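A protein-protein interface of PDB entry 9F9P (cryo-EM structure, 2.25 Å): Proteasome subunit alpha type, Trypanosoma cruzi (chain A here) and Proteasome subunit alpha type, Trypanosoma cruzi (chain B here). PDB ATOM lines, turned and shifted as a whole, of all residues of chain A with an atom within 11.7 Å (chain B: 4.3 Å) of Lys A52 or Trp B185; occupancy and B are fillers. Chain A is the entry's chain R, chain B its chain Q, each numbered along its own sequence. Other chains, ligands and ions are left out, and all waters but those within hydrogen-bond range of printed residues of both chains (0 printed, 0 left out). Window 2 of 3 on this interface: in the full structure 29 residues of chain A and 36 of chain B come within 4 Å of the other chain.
Lys A52 touches three residues of chain B. Of the printed residues of chain B, Leu A53 touches Arg B166 (2.9 Å) and Ala B167 (3.9 Å). Of the printed residues of chain B, Asp A55 touches Leu B38. Printed residues of chain B within 4 Å of Ser A56: Arg B166 (3.97 Å). No residue of chain A comes within 4 Å of Ile B37. Leu B38 touches one residue of chain A. Of chain A, only Leu A53 comes within 4 Å of Ala B167. Leu B181 touches none of the printed residues of chain A. Lys B182 touches one residue of chain A. Arg B183 touches none of the printed residues of chain A. No residue of chain A comes within 4 Å of Asp B184. Trp B185 touches just one residue of chain A: Lys A52 (3.3 Å). No residue of chain A comes within 4 Å of Lys B186. No residue of chain A comes within 4 Å of Pro B187. The nearest printed residue of chain B that does not touch Lys A52 is Arg B183 (4.7 Å). The nearest residue of chain A that does not touch Trp B185 is Leu A53 (4.6 Å). The nearest printed residue of chain B that does not touch Gln A54 is Ala B167 (5.8 Å).
The backbone carbonyl oxygen (O) of Trp B185 lies within hydrogen-bond range of the side-chain amino group (NZ) of Lys A52 (3.3 Å). The backbone NH (N) of Arg B166 is in hydrogen-bond range of the backbone carbonyl oxygen (O) of Leu A53 (2.9 Å). The backbone carbonyl oxygen (O) of Lys A52 sits at hydrogen-bond distance from the guanidinium group (NH1) of Arg B166, at 2.8 Å. The guanidinium group (NE) of Arg B166 lies close to the backbone carbonyl oxygen (O) of Gln A54, 3.4 Å away.
The backbone NH (N) of Leu B38 is in hydrogen-bond range of the backbone carbonyl oxygen (O) of Arg B166. O of Leu B38 lies within hydrogen-bond range of NE1 of Trp B185 (3.2 Å).
Of the 13 printed residues of chain A, 5 touch a printed residue of chain B. Along chain B the printed residues that touch a printed residue of chain A span positions 38 to 185. Among the printed residues, no Asp or Glu carboxylate lies within 4 Å of a Lys or Arg side-chain nitrogen of the other chain.
Among the printed residues, pairs that only touch across the chains: Lys A52 with Lys B182 (3.0 Å), Leu A53 with Ala B167 (3.9 Å), Asp A55 with Leu B38 (3.9 Å) and Ser A56 with Arg B166 (3.97 Å).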
ATOM      1  N   LYS A  48     -29.379  14.096 -25.809  1.00  0.00           N
ATOM      2  CA  LYS A  48     -30.709  13.510 -25.674  1.00  0.00           C
ATOM      3  C   LYS A  48     -31.632  14.390 -24.832  1.00  0.00           C
ATOM      4  O   LYS A  48     -32.778  14.608 -25.216  1.00  0.00           O
ATOM      5  CB  LYS A  48     -30.602  12.088 -25.106  1.00  0.00           C
ATOM      6  CG  LYS A  48     -30.046  11.058 -26.090  1.00  0.00           C
ATOM      7  CD  LYS A  48     -29.391   9.813 -25.484  1.00  0.00           C
ATOM      8  CE  LYS A  48     -30.293   8.598 -25.401  1.00  0.00           C
ATOM      9  NZ  LYS A  48     -31.264   8.698 -24.286  1.00  0.00           N
ATOM     10  N   SER A  49     -31.128  14.878 -23.692  1.00  0.00           N
ATOM     11  CA  SER A  49     -31.879  15.758 -22.807  1.00  0.00           C
ATOM     12  C   SER A  49     -31.162  15.874 -21.465  1.00  0.00           C
ATOM     13  O   SER A  49     -30.269  15.081 -21.158  1.00  0.00           O
ATOM     14  CB  SER A  49     -33.308  15.295 -22.602  1.00  0.00           C
ATOM     15  OG  SER A  49     -34.161  15.778 -23.632  1.00  0.00           O
ATOM     16  N   VAL A  50     -31.585  16.866 -20.672  1.00  0.00           N
ATOM     17  CA  VAL A  50     -31.075  17.076 -19.327  1.00  0.00           C
ATOM     18  C   VAL A  50     -31.965  16.320 -18.340  1.00  0.00           C
ATOM     19  O   VAL A  50     -33.191  16.371 -18.433  1.00  0.00           O
ATOM     20  CB  VAL A  50     -31.003  18.578 -18.981  1.00  0.00           C
ATOM     21  CG1 VAL A  50     -30.767  18.820 -17.495  1.00  0.00           C
ATOM     22  CG2 VAL A  50     -29.954  19.289 -19.822  1.00  0.00           C
ATOM     23  N   GLN A  51     -31.324  15.628 -17.393  1.00  0.00           N
ATOM     24  CA  GLN A  51     -32.021  14.884 -16.359  1.00  0.00           C
ATOM     25  C   GLN A  51     -31.265  15.040 -15.045  1.00  0.00           C
ATOM     26  O   GLN A  51     -30.075  15.349 -15.039  1.00  0.00           O
ATOM     27  CB  GLN A  51     -32.108  13.403 -16.727  1.00  0.00           C
ATOM     28  CG  GLN A  51     -32.743  13.146 -18.084  1.00  0.00           C
ATOM     29  CD  GLN A  51     -33.368  11.778 -18.152  1.00  0.00           C
ATOM     30  OE1 GLN A  51     -34.117  11.374 -17.267  1.00  0.00           O
ATOM     31  NE2 GLN A  51     -33.072  11.050 -19.214  1.00  0.00           N
ATOM     32  N   LYS A  52     -31.960  14.811 -13.929  1.00  0.00           N
ATOM     33  CA  LYS A  52     -31.306  14.864 -12.635  1.00  0.00           C
ATOM     34  C   LYS A  52     -30.492  13.581 -12.437  1.00  0.00           C
ATOM     35  O   LYS A  52     -29.448  13.606 -11.783  1.00  0.00           O
ATOM     36  CB  LYS A  52     -32.347  15.107 -11.536  1.00  0.00           C
ATOM     37  CG  LYS A  52     -31.769  15.229 -10.128  1.00  0.00           C
ATOM     38  CD  LYS A  52     -32.804  15.339  -9.012  1.00  0.00           C
ATOM     39  CE  LYS A  52     -32.406  14.591  -7.752  1.00  0.00           C
ATOM     40  NZ  LYS A  52     -31.091  15.021  -7.221  1.00  0.00           N
ATOM     41  N   LEU A  53     -30.957  12.481 -13.060  1.00  0.00           N
ATOM     42  CA  LEU A  53     -30.475  11.131 -12.797  1.00  0.00           C
ATOM     43  C   LEU A  53     -29.332  10.713 -13.717  1.00  0.00           C
ATOM     44  O   LEU A  53     -28.655   9.737 -13.408  1.00  0.00           O
ATOM     45  CB  LEU A  53     -31.638  10.167 -13.003  1.00  0.00           C
ATOM     46  CG  LEU A  53     -32.691  10.169 -11.902  1.00  0.00           C
ATOM     47  CD1 LEU A  53     -33.781   9.161 -12.230  1.00  0.00           C
ATOM     48  CD2 LEU A  53     -32.071   9.880 -10.540  1.00  0.00           C
ATOM     49  N   GLN A  54     -29.153  11.404 -14.852  1.00  0.00           N
ATOM     50  CA  GLN A  54     -28.064  11.100 -15.766  1.00  0.00           C
ATOM     51  C   GLN A  54     -26.749  11.262 -15.015  1.00  0.00           C
ATOM     52  O   GLN A  54     -26.669  12.069 -14.094  1.00  0.00           O
ATOM     53  CB  GLN A  54     -28.061  12.056 -16.964  1.00  0.00           C
ATOM     54  CG  GLN A  54     -27.427  11.485 -18.227  1.00  0.00           C
ATOM     55  CD  GLN A  54     -28.419  10.690 -19.048  1.00  0.00           C
ATOM     56  OE1 GLN A  54     -29.272  11.255 -19.731  1.00  0.00           O
ATOM     57  NE2 GLN A  54     -28.326   9.369 -18.987  1.00  0.00           N
ATOM     58  N   ASP A  55     -25.726  10.501 -15.413  1.00  0.00           N
ATOM     59  CA  ASP A  55     -24.401  10.630 -14.829  1.00  0.00           C
ATOM     60  C   ASP A  55     -23.691  11.796 -15.516  1.00  0.00           C
ATOM     61  O   ASP A  55     -23.708  11.906 -16.748  1.00  0.00           O
ATOM     62  CB  ASP A  55     -23.622   9.307 -14.896  1.00  0.00           C
ATOM     63  CG  ASP A  55     -22.320   9.236 -14.100  1.00  0.00           C
ATOM     64  OD1 ASP A  55     -21.253   9.230 -14.733  1.00  0.00           O
ATOM     65  OD2 ASP A  55     -22.377   9.139 -12.850  1.00  0.00           O
ATOM     66  N   SER A  56     -23.078  12.651 -14.671  1.00  0.00           N
ATOM     67  CA  SER A  56     -22.363  13.859 -15.067  1.00  0.00           C
ATOM     68  C   SER A  56     -21.312  13.550 -16.131  1.00  0.00           C
ATOM     69  O   SER A  56     -21.288  14.218 -17.165  1.00  0.00           O
ATOM     70  CB  SER A  56     -21.746  14.536 -13.867  1.00  0.00           C
ATOM     71  OG  SER A  56     -20.981  13.615 -13.102  1.00  0.00           O
ATOM     72  N   ARG A  57     -20.442  12.554 -15.885  1.00  0.00           N
ATOM     73  CA  ARG A  57     -19.538  12.113 -16.934  1.00  0.00           C
ATOM     74  C   ARG A  57     -20.387  11.514 -18.046  1.00  0.00           C
ATOM     75  O   ARG A  57     -20.809  10.363 -17.969  1.00  0.00           O
ATOM     76  CB  ARG A  57     -18.485  11.089 -16.493  1.00  0.00           C
ATOM     77  CG  ARG A  57     -17.622  10.632 -17.667  1.00  0.00           C
ATOM     78  CD  ARG A  57     -16.737   9.434 -17.384  1.00  0.00           C
ATOM     79  NE  ARG A  57     -17.420   8.144 -17.273  1.00  0.00           N
ATOM     80  CZ  ARG A  57     -17.837   7.403 -18.296  1.00  0.00           C
ATOM     81  NH1 ARG A  57     -18.333   6.204 -18.063  1.00  0.00           N
ATOM     82  NH2 ARG A  57     -17.741   7.842 -19.539  1.00  0.00           N
ATOM     83  N   THR A  58     -20.635  12.314 -19.081  1.00  0.00           N
ATOM     84  CA  THR A  58     -21.467  11.874 -20.186  1.00  0.00           C
ATOM     85  C   THR A  58     -20.639  10.991 -21.125  1.00  0.00           C
ATOM     86  O   THR A  58     -19.435  11.193 -21.298  1.00  0.00           O
ATOM     87  CB  THR A  58     -22.133  13.083 -20.858  1.00  0.00           C
ATOM     88  OG1 THR A  58     -21.100  13.920 -21.385  1.00  0.00           O
ATOM     89  CG2 THR A  58     -23.009  13.872 -19.903  1.00  0.00           C
ATOM     90  N   SER A 201     -28.291  24.588 -22.396  1.00  0.00           N
ATOM     91  CA  SER A 201     -27.676  24.286 -21.113  1.00  0.00           C
ATOM     92  C   SER A 201     -26.721  23.100 -21.267  1.00  0.00           C
ATOM     93  O   SER A 201     -25.609  23.272 -21.765  1.00  0.00           O
ATOM     94  CB  SER A 201     -28.739  24.058 -20.062  1.00  0.00           C
ATOM     95  OG  SER A 201     -28.170  23.577 -18.853  1.00  0.00           O
ATOM     96  N   LYS A 202     -27.160  21.905 -20.844  1.00  0.00           N
ATOM     97  CA  LYS A 202     -26.393  20.681 -21.034  1.00  0.00           C
ATOM     98  C   LYS A 202     -27.058  19.830 -22.117  1.00  0.00           C
ATOM     99  O   LYS A 202     -27.222  18.624 -21.944  1.00  0.00           O
ATOM    100  CB  LYS A 202     -26.285  19.890 -19.724  1.00  0.00           C
ATOM    101  CG  LYS A 202     -25.606  20.602 -18.559  1.00  0.00           C
ATOM    102  CD  LYS A 202     -25.661  19.810 -17.266  1.00  0.00           C
ATOM    103  CE  LYS A 202     -25.029  20.531 -16.095  1.00  0.00           C
ATOM    104  NZ  LYS A 202     -25.236  19.794 -14.826  1.00  0.00           N
ATOM    105  N   ILE B  37     -28.650   1.827  -7.892  1.00  0.00           N
ATOM    106  CA  ILE B  37     -28.322   3.098  -7.228  1.00  0.00           C
ATOM    107  C   ILE B  37     -26.818   3.280  -7.017  1.00  0.00           C
ATOM    108  O   ILE B  37     -26.154   2.426  -6.476  1.00  0.00           O
ATOM    109  CB  ILE B  37     -29.089   3.185  -5.896  1.00  0.00           C
ATOM    110  CG1 ILE B  37     -30.592   3.248  -6.142  1.00  0.00           C
ATOM    111  CG2 ILE B  37     -28.666   4.389  -5.068  1.00  0.00           C
ATOM    112  CD1 ILE B  37     -31.388   2.997  -4.889  1.00  0.00           C
ATOM    113  N   LEU B  38     -26.279   4.415  -7.425  1.00  0.00           N
ATOM    114  CA  LEU B  38     -24.871   4.754  -7.229  1.00  0.00           C
ATOM    115  C   LEU B  38     -24.672   5.548  -5.935  1.00  0.00           C
ATOM    116  O   LEU B  38     -25.227   6.631  -5.799  1.00  0.00           O
ATOM    117  CB  LEU B  38     -24.464   5.610  -8.433  1.00  0.00           C
ATOM    118  CG  LEU B  38     -22.976   5.862  -8.655  1.00  0.00           C
ATOM    119  CD1 LEU B  38     -22.343   4.673  -9.332  1.00  0.00           C
ATOM    120  CD2 LEU B  38     -22.751   7.087  -9.533  1.00  0.00           C
ATOM    121  N   ARG B 166     -26.946   7.682 -12.377  1.00  0.00           N
ATOM    122  CA  ARG B 166     -26.764   7.778 -10.939  1.00  0.00           C
ATOM    123  C   ARG B 166     -27.820   6.933 -10.247  1.00  0.00           C
ATOM    124  O   ARG B 166     -27.575   6.387  -9.191  1.00  0.00           O
ATOM    125  CB  ARG B 166     -26.938   9.229 -10.472  1.00  0.00           C
ATOM    126  CG  ARG B 166     -25.877  10.208 -10.967  1.00  0.00           C
ATOM    127  CD  ARG B 166     -26.409  11.629 -10.876  1.00  0.00           C
ATOM    128  NE  ARG B 166     -25.387  12.662 -11.018  1.00  0.00           N
ATOM    129  CZ  ARG B 166     -25.648  13.969 -11.036  1.00  0.00           C
ATOM    130  NH1 ARG B 166     -26.891  14.395 -10.896  1.00  0.00           N
ATOM    131  NH2 ARG B 166     -24.670  14.842 -11.204  1.00  0.00           N
ATOM    132  N   ALA B 167     -28.993   6.816 -10.862  1.00  0.00           N
ATOM    133  CA  ALA B 167     -29.957   5.807 -10.444  1.00  0.00           C
ATOM    134  C   ALA B 167     -30.855   5.493 -11.621  1.00  0.00           C
ATOM    135  O   ALA B 167     -30.957   6.367 -12.489  1.00  0.00           O
ATOM    136  CB  ALA B 167     -30.760   6.303  -9.296  1.00  0.00           C
ATOM    137  N   LEU B 181     -37.036   8.015  -7.294  1.00  0.00           N
ATOM    138  CA  LEU B 181     -35.586   8.144  -7.241  1.00  0.00           C
ATOM    139  C   LEU B 181     -35.169   9.574  -7.572  1.00  0.00           C
ATOM    140  O   LEU B 181     -34.255  10.093  -6.941  1.00  0.00           O
ATOM    141  CB  LEU B 181     -34.927   7.155  -8.212  1.00  0.00           C
ATOM    142  CG  LEU B 181     -35.007   5.694  -7.788  1.00  0.00           C
ATOM    143  CD1 LEU B 181     -34.792   4.774  -8.978  1.00  0.00           C
ATOM    144  CD2 LEU B 181     -33.999   5.397  -6.692  1.00  0.00           C
ATOM    145  N   LYS B 182     -35.845  10.200  -8.544  1.00  0.00           N
ATOM    146  CA  LYS B 182     -35.562  11.576  -8.936  1.00  0.00           C
ATOM    147  C   LYS B 182     -35.786  12.538  -7.763  1.00  0.00           C
ATOM    148  O   LYS B 182     -35.240  13.633  -7.756  1.00  0.00           O
ATOM    149  CB  LYS B 182     -36.415  11.961 -10.154  1.00  0.00           C
ATOM    150  CG  LYS B 182     -36.238  13.390 -10.657  1.00  0.00           C
ATOM    151  CD  LYS B 182     -36.877  13.668 -12.010  1.00  0.00           C
ATOM    152  CE  LYS B 182     -36.015  13.227 -13.177  1.00  0.00           C
ATOM    153  NZ  LYS B 182     -36.503  13.781 -14.461  1.00  0.00           N
ATOM    154  N   ARG B 183     -36.575  12.136  -6.764  1.00  0.00           N
ATOM    155  CA  ARG B 183     -36.817  12.964  -5.594  1.00  0.00           C
ATOM    156  C   ARG B 183     -35.751  12.719  -4.517  1.00  0.00           C
ATOM    157  O   ARG B 183     -35.124  13.676  -4.072  1.00  0.00           O
ATOM    158  CB  ARG B 183     -38.240  12.702  -5.097  1.00  0.00           C
ATOM    159  CG  ARG B 183     -38.761  13.726  -4.099  1.00  0.00           C
ATOM    160  CD  ARG B 183     -40.281  13.745  -4.045  1.00  0.00           C
ATOM    161  NE  ARG B 183     -40.894  12.437  -3.826  1.00  0.00           N
ATOM    162  CZ  ARG B 183     -40.789  11.719  -2.708  1.00  0.00           C
ATOM    163  NH1 ARG B 183     -40.007  12.128  -1.725  1.00  0.00           N
ATOM    164  NH2 ARG B 183     -41.460  10.586  -2.578  1.00  0.00           N
ATOM    165  N   ASP B 184     -35.501  11.449  -4.148  1.00  0.00           N
ATOM    166  CA  ASP B 184     -34.767  11.091  -2.935  1.00  0.00           C
ATOM    167  C   ASP B 184     -33.294  10.712  -3.146  1.00  0.00           C
ATOM    168  O   ASP B 184     -32.652  10.287  -2.187  1.00  0.00           O
ATOM    169  CB  ASP B 184     -35.412   9.898  -2.223  1.00  0.00           C
ATOM    170  CG  ASP B 184     -36.831  10.156  -1.747  1.00  0.00           C
ATOM    171  OD1 ASP B 184     -37.730   9.368  -2.123  1.00  0.00           O
ATOM    172  OD2 ASP B 184     -37.030  11.143  -1.001  1.00  0.00           O
ATOM    173  N   TRP B 185     -32.748  10.825  -4.359  1.00  0.00           N
ATOM    174  CA  TRP B 185     -31.337  10.541  -4.580  1.00  0.00           C
ATOM    175  C   TRP B 185     -30.543  11.814  -4.287  1.00  0.00           C
ATOM    176  O   TRP B 185     -31.003  12.905  -4.626  1.00  0.00           O
ATOM    177  CB  TRP B 185     -31.059  10.049  -6.025  1.00  0.00           C
ATOM    178  CG  TRP B 185     -29.624   9.670  -6.280  1.00  0.00           C
ATOM    179  CD1 TRP B 185     -29.054   8.442  -6.075  1.00  0.00           C
ATOM    180  CD2 TRP B 185     -28.547  10.533  -6.708  1.00  0.00           C
ATOM    181  NE1 TRP B 185     -27.717   8.476  -6.375  1.00  0.00           N
ATOM    182  CE2 TRP B 185     -27.374   9.745  -6.749  1.00  0.00           C
ATOM    183  CE3 TRP B 185     -28.452  11.893  -7.030  1.00  0.00           C
ATOM    184  CZ2 TRP B 185     -26.134  10.265  -7.114  1.00  0.00           C
ATOM    185  CZ3 TRP B 185     -27.222  12.420  -7.381  1.00  0.00           C
ATOM    186  CH2 TRP B 185     -26.081  11.610  -7.421  1.00  0.00           C
ATOM    187  N   LYS B 186     -29.331  11.657  -3.729  1.00  0.00           N
ATOM    188  CA  LYS B 186     -28.456  12.788  -3.432  1.00  0.00           C
ATOM    189  C   LYS B 186     -26.991  12.356  -3.520  1.00  0.00           C
ATOM    190  O   LYS B 186     -26.665  11.200  -3.258  1.00  0.00           O
ATOM    191  CB  LYS B 186     -28.806  13.402  -2.068  1.00  0.00           C
ATOM    192  CG  LYS B 186     -28.854  12.418  -0.906  1.00  0.00           C
ATOM    193  CD  LYS B 186     -30.162  12.456  -0.108  1.00  0.00           C
ATOM    194  CE  LYS B 186     -30.366  13.726   0.689  1.00  0.00           C
ATOM    195  NZ  LYS B 186     -29.282  13.925   1.680  1.00  0.00           N
ATOM    196  N   PRO B 187     -26.072  13.282  -3.897  1.00  0.00           N
ATOM    197  CA  PRO B 187     -24.659  12.952  -4.128  1.00  0.00           C
ATOM    198  C   PRO B 187     -23.854  12.408  -2.950  1.00  0.00           C
ATOM    199  O   PRO B 187     -22.712  11.992  -3.136  1.00  0.00           O
ATOM    200  CB  PRO B 187     -23.988  14.284  -4.509  1.00  0.00           C
ATOM    201  CG  PRO B 187     -25.138  15.220  -4.885  1.00  0.00           C
ATOM    202  CD  PRO B 187     -26.361  14.705  -4.148  1.00  0.00           C
ATOM    203  N   LEU B 189     -24.771   9.954  -0.516  1.00  0.00           N
ATOM    204  CA  LEU B 189     -25.390   8.769   0.071  1.00  0.00           C
ATOM    205  C   LEU B 189     -24.314   7.770   0.485  1.00  0.00           C
ATOM    206  O   LEU B 189     -23.307   7.628  -0.205  1.00  0.00           O
ATOM    207  CB  LEU B 189     -26.306   8.097  -0.962  1.00  0.00           C
ATOM    208  CG  LEU B 189     -27.794   8.455  -0.980  1.00  0.00           C
ATOM    209  CD1 LEU B 189     -28.472   7.771  -2.155  1.00  0.00           C
ATOM    210  CD2 LEU B 189     -28.491   8.033   0.295  1.00  0.00           C
